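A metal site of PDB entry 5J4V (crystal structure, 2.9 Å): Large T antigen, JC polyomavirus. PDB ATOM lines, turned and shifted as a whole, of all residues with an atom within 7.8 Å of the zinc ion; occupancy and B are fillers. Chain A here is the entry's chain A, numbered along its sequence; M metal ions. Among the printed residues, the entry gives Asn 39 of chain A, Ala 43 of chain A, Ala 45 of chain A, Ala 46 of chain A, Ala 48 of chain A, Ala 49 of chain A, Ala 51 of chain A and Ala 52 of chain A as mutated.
A ring nitrogen (NE2) of His 62 is in hydrogen-bond range of the backbone carbonyl oxygen (O) of Phe 40, 3.0 Å away.
A ring nitrogen (NE2) of His 62 sits at hydrogen-bond distance from the backbone carbonyl oxygen (O) of Glu 42 (2.7 Å).
The side-chain sulfur of Cys 47 lies close to the backbone NH of Ala 49 (3.5 Å).
Four residues have an atom within 4 Å of the zinc ion: Cys 47, Cys 50, His 58 and His 62.
The nearest printed residue that does not touch the zinc ion is Ala 49 (4.4 Å).
The zinc ion is bound by ND1 of His 62, at 2.0 Å.
SG of Cys 50 is bound to the zinc ion, at 2.2 Å.
A ring nitrogen (NE2) of His 58 binds the zinc ion, at 2.3 Å.
SG of Cys 47 binds the zinc ion, at 2.4 Å.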
ATOM      1  N   ASN A  39     -22.049 -11.242  10.242  1.00  0.00           N
ATOM      2  CA  ASN A  39     -23.250 -12.030  10.515  1.00  0.00           C
ATOM      3  C   ASN A  39     -23.036 -13.199  11.500  1.00  0.00           C
ATOM      4  O   ASN A  39     -24.009 -13.748  12.031  1.00  0.00           O
ATOM      5  CB  ASN A  39     -23.907 -12.506   9.221  1.00  0.00           C
ATOM      6  CG  ASN A  39     -24.620 -11.441   8.430  1.00  0.00           C
ATOM      7  OD1 ASN A  39     -24.868 -10.327   8.903  1.00  0.00           O
ATOM      8  ND2 ASN A  39     -25.004 -11.796   7.229  1.00  0.00           N
ATOM      9  N   PHE A  40     -21.745 -13.511  11.786  1.00  0.00           N
ATOM     10  CA  PHE A  40     -21.309 -14.578  12.695  1.00  0.00           C
ATOM     11  C   PHE A  40     -21.245 -14.144  14.173  1.00  0.00           C
ATOM     12  O   PHE A  40     -20.962 -14.992  15.021  1.00  0.00           O
ATOM     13  CB  PHE A  40     -19.917 -15.098  12.273  1.00  0.00           C
ATOM     14  CG  PHE A  40     -19.761 -15.777  10.929  1.00  0.00           C
ATOM     15  CD1 PHE A  40     -20.773 -16.590  10.412  1.00  0.00           C
ATOM     16  CD2 PHE A  40     -18.563 -15.695  10.232  1.00  0.00           C
ATOM     17  CE1 PHE A  40     -20.607 -17.238   9.186  1.00  0.00           C
ATOM     18  CE2 PHE A  40     -18.390 -16.366   9.010  1.00  0.00           C
ATOM     19  CZ  PHE A  40     -19.412 -17.120   8.495  1.00  0.00           C
ATOM     20  N   GLU A  42     -23.717 -13.008  16.209  1.00  0.00           N
ATOM     21  CA  GLU A  42     -24.879 -13.498  16.962  1.00  0.00           C
ATOM     22  C   GLU A  42     -24.688 -14.979  17.357  1.00  0.00           C
ATOM     23  O   GLU A  42     -23.914 -15.678  16.707  1.00  0.00           O
ATOM     24  CB  GLU A  42     -26.179 -13.307  16.147  1.00  0.00           C
ATOM     25  CG  GLU A  42     -26.441 -11.866  15.742  1.00  0.00           C
ATOM     26  CD  GLU A  42     -26.867 -10.954  16.878  1.00  0.00           C
ATOM     27  OE1 GLU A  42     -28.029 -11.086  17.350  1.00  0.00           O
ATOM     28  OE2 GLU A  42     -26.053 -10.105  17.292  1.00  0.00           O
ATOM     29  N   ALA A  43     -25.338 -15.432  18.453  1.00  0.00           N
ATOM     30  CA  ALA A  43     -25.199 -16.809  18.962  1.00  0.00           C
ATOM     31  C   ALA A  43     -25.717 -17.895  17.988  1.00  0.00           C
ATOM     32  O   ALA A  43     -26.886 -17.831  17.588  1.00  0.00           O
ATOM     33  CB  ALA A  43     -25.838 -16.937  20.331  1.00  0.00           C
ATOM     34  N   PRO A  44     -24.867 -18.890  17.581  1.00  0.00           N
ATOM     35  CA  PRO A  44     -25.339 -19.919  16.627  1.00  0.00           C
ATOM     36  C   PRO A  44     -26.531 -20.725  17.113  1.00  0.00           C
ATOM     37  O   PRO A  44     -27.400 -21.072  16.310  1.00  0.00           O
ATOM     38  CB  PRO A  44     -24.102 -20.794  16.389  1.00  0.00           C
ATOM     39  CG  PRO A  44     -22.946 -19.960  16.802  1.00  0.00           C
ATOM     40  CD  PRO A  44     -23.456 -19.104  17.938  1.00  0.00           C
ATOM     41  N   ALA A  45     -26.597 -20.973  18.440  1.00  0.00           N
ATOM     42  CA  ALA A  45     -27.674 -21.711  19.109  1.00  0.00           C
ATOM     43  C   ALA A  45     -29.040 -21.072  18.898  1.00  0.00           C
ATOM     44  O   ALA A  45     -30.038 -21.793  18.822  1.00  0.00           O
ATOM     45  CB  ALA A  45     -27.386 -21.848  20.591  1.00  0.00           C
ATOM     46  N   ALA A  46     -29.092 -19.724  18.771  1.00  0.00           N
ATOM     47  CA  ALA A  46     -30.312 -18.966  18.526  1.00  0.00           C
ATOM     48  C   ALA A  46     -30.279 -18.316  17.130  1.00  0.00           C
ATOM     49  O   ALA A  46     -30.952 -17.301  16.894  1.00  0.00           O
ATOM     50  CB  ALA A  46     -30.474 -17.907  19.594  1.00  0.00           C
ATOM     51  N   CYS A  47     -29.483 -18.882  16.207  1.00  0.00           N
ATOM     52  CA  CYS A  47     -29.350 -18.329  14.854  1.00  0.00           C
ATOM     53  C   CYS A  47     -30.322 -18.945  13.861  1.00  0.00           C
ATOM     54  O   CYS A  47     -30.274 -20.156  13.607  1.00  0.00           O
ATOM     55  CB  CYS A  47     -27.909 -18.389  14.356  1.00  0.00           C
ATOM     56  SG  CYS A  47     -27.693 -17.847  12.637  1.00  0.00           S
ATOM     57  N   ALA A  48     -31.176 -18.081  13.266  1.00  0.00           N
ATOM     58  CA  ALA A  48     -32.174 -18.495  12.284  1.00  0.00           C
ATOM     59  C   ALA A  48     -31.567 -18.975  10.961  1.00  0.00           C
ATOM     60  O   ALA A  48     -32.110 -19.898  10.366  1.00  0.00           O
ATOM     61  CB  ALA A  48     -33.156 -17.367  12.037  1.00  0.00           C
ATOM     62  N   ALA A  49     -30.451 -18.353  10.513  1.00  0.00           N
ATOM     63  CA  ALA A  49     -29.749 -18.734   9.279  1.00  0.00           C
ATOM     64  C   ALA A  49     -29.043 -20.087   9.449  1.00  0.00           C
ATOM     65  O   ALA A  49     -28.775 -20.767   8.464  1.00  0.00           O
ATOM     66  CB  ALA A  49     -28.750 -17.660   8.876  1.00  0.00           C
ATOM     67  N   CYS A  50     -28.776 -20.470  10.715  1.00  0.00           N
ATOM     68  CA  CYS A  50     -28.175 -21.738  11.112  1.00  0.00           C
ATOM     69  C   CYS A  50     -29.252 -22.795  11.079  1.00  0.00           C
ATOM     70  O   CYS A  50     -29.017 -23.897  10.580  1.00  0.00           O
ATOM     71  CB  CYS A  50     -27.526 -21.646  12.486  1.00  0.00           C
ATOM     72  SG  CYS A  50     -25.740 -21.382  12.453  1.00  0.00           S
ATOM     73  N   ALA A  51     -30.465 -22.457  11.624  1.00  0.00           N
ATOM     74  CA  ALA A  51     -31.645 -23.323  11.680  1.00  0.00           C
ATOM     75  C   ALA A  51     -32.178 -23.634  10.250  1.00  0.00           C
ATOM     76  O   ALA A  51     -32.559 -24.776   9.985  1.00  0.00           O
ATOM     77  CB  ALA A  51     -32.735 -22.667  12.512  1.00  0.00           C
ATOM     78  N   ALA A  52     -32.120 -22.607   9.342  1.00  0.00           N
ATOM     79  CA  ALA A  52     -32.531 -22.688   7.924  1.00  0.00           C
ATOM     80  C   ALA A  52     -31.600 -23.588   7.109  1.00  0.00           C
ATOM     81  O   ALA A  52     -32.068 -24.278   6.192  1.00  0.00           O
ATOM     82  CB  ALA A  52     -32.570 -21.299   7.311  1.00  0.00           C
ATOM     83  N   GLN A  55     -27.287 -21.523   3.579  1.00  0.00           N
ATOM     84  CA  GLN A  55     -26.116 -20.725   3.211  1.00  0.00           C
ATOM     85  C   GLN A  55     -24.904 -21.455   3.797  1.00  0.00           C
ATOM     86  O   GLN A  55     -24.561 -21.167   4.944  1.00  0.00           O
ATOM     87  CB  GLN A  55     -26.246 -19.308   3.782  1.00  0.00           C
ATOM     88  CG  GLN A  55     -26.684 -18.248   2.778  1.00  0.00           C
ATOM     89  CD  GLN A  55     -26.016 -16.913   3.082  1.00  0.00           C
ATOM     90  OE1 GLN A  55     -25.823 -16.525   4.241  1.00  0.00           O
ATOM     91  NE2 GLN A  55     -25.615 -16.196   2.028  1.00  0.00           N
ATOM     92  N   HIS A  58     -22.237 -19.660   5.542  1.00  0.00           N
ATOM     93  CA  HIS A  58     -22.620 -19.196   6.861  1.00  0.00           C
ATOM     94  C   HIS A  58     -22.785 -20.245   7.988  1.00  0.00           C
ATOM     95  O   HIS A  58     -22.316 -20.002   9.098  1.00  0.00           O
ATOM     96  CB  HIS A  58     -23.955 -18.439   6.799  1.00  0.00           C
ATOM     97  CG  HIS A  58     -24.568 -18.258   8.154  1.00  0.00           C
ATOM     98  ND1 HIS A  58     -24.111 -17.280   9.030  1.00  0.00           N
ATOM     99  CD2 HIS A  58     -25.494 -19.007   8.785  1.00  0.00           C
ATOM    100  CE1 HIS A  58     -24.825 -17.425  10.133  1.00  0.00           C
ATOM    101  NE2 HIS A  58     -25.645 -18.466  10.042  1.00  0.00           N
ATOM    102  N   PHE A  59     -23.489 -21.380   7.717  1.00  0.00           N
ATOM    103  CA  PHE A  59     -23.835 -22.417   8.703  1.00  0.00           C
ATOM    104  C   PHE A  59     -22.662 -23.370   8.935  1.00  0.00           C
ATOM    105  O   PHE A  59     -22.571 -23.951  10.021  1.00  0.00           O
ATOM    106  CB  PHE A  59     -25.126 -23.207   8.381  1.00  0.00           C
ATOM    107  CG  PHE A  59     -25.153 -24.107   7.156  1.00  0.00           C
ATOM    108  CD1 PHE A  59     -24.493 -25.330   7.161  1.00  0.00           C
ATOM    109  CD2 PHE A  59     -25.936 -23.780   6.064  1.00  0.00           C
ATOM    110  CE1 PHE A  59     -24.541 -26.179   6.044  1.00  0.00           C
ATOM    111  CE2 PHE A  59     -25.996 -24.629   4.950  1.00  0.00           C
ATOM    112  CZ  PHE A  59     -25.299 -25.819   4.952  1.00  0.00           C
ATOM    113  N   ASN A  60     -21.763 -23.522   7.955  1.00  0.00           N
ATOM    114  CA  ASN A  60     -20.604 -24.380   8.187  1.00  0.00           C
ATOM    115  C   ASN A  60     -19.522 -23.639   8.946  1.00  0.00           C
ATOM    116  O   ASN A  60     -18.629 -24.259   9.511  1.00  0.00           O
ATOM    117  CB  ASN A  60     -20.006 -24.895   6.870  1.00  0.00           C
ATOM    118  CG  ASN A  60     -20.822 -25.944   6.151  1.00  0.00           C
ATOM    119  OD1 ASN A  60     -21.451 -26.843   6.758  1.00  0.00           O
ATOM    120  ND2 ASN A  60     -20.767 -25.883   4.835  1.00  0.00           N
ATOM    121  N   HIS A  61     -19.603 -22.320   8.977  1.00  0.00           N
ATOM    122  CA  HIS A  61     -18.564 -21.529   9.577  1.00  0.00           C
ATOM    123  C   HIS A  61     -18.981 -20.798  10.857  1.00  0.00           C
ATOM    124  O   HIS A  61     -18.115 -20.465  11.658  1.00  0.00           O
ATOM    125  CB  HIS A  61     -17.995 -20.577   8.514  1.00  0.00           C
ATOM    126  CG  HIS A  61     -17.568 -21.286   7.267  1.00  0.00           C
ATOM    127  ND1 HIS A  61     -16.273 -21.786   7.123  1.00  0.00           N
ATOM    128  CD2 HIS A  61     -18.284 -21.611   6.160  1.00  0.00           C
ATOM    129  CE1 HIS A  61     -16.240 -22.366   5.929  1.00  0.00           C
ATOM    130  NE2 HIS A  61     -17.425 -22.290   5.316  1.00  0.00           N
ATOM    131  N   HIS A  62     -20.281 -20.576  11.089  1.00  0.00           N
ATOM    132  CA  HIS A  62     -20.776 -19.842  12.263  1.00  0.00           C
ATOM    133  C   HIS A  62     -20.189 -20.314  13.605  1.00  0.00           C
ATOM    134  O   HIS A  62     -19.758 -19.472  14.390  1.00  0.00           O
ATOM    135  CB  HIS A  62     -22.315 -19.806  12.322  1.00  0.00           C
ATOM    136  CG  HIS A  62     -22.868 -18.656  13.113  1.00  0.00           C
ATOM    137  ND1 HIS A  62     -24.229 -18.372  13.110  1.00  0.00           N
ATOM    138  CD2 HIS A  62     -22.243 -17.775  13.932  1.00  0.00           C
ATOM    139  CE1 HIS A  62     -24.381 -17.323  13.903  1.00  0.00           C
ATOM    140  NE2 HIS A  62     -23.215 -16.938  14.423  1.00  0.00           N
ATOM    141  N   GLU A  63     -20.170 -21.623  13.882  1.00  0.00           N
ATOM    142  CA  GLU A  63     -19.638 -22.100  15.153  1.00  0.00           C
ATOM    143  C   GLU A  63     -18.127 -21.846  15.340  1.00  0.00           C
ATOM    144  O   GLU A  63     -17.705 -21.486  16.428  1.00  0.00           O
ATOM    145  CB  GLU A  63     -20.004 -23.563  15.391  1.00  0.00           C
ATOM    146  CG  GLU A  63     -21.466 -23.722  15.783  1.00  0.00           C
ATOM    147  CD  GLU A  63     -21.891 -24.986  16.518  1.00  0.00           C
ATOM    148  OE1 GLU A  63     -21.135 -25.988  16.466  1.00  0.00           O
ATOM    149  OE2 GLU A  63     -22.991 -24.977  17.114  1.00  0.00           O
HETATM  150 ZN    ZN M   1     -25.783 -19.161  12.204  1.00  0.00          ZN
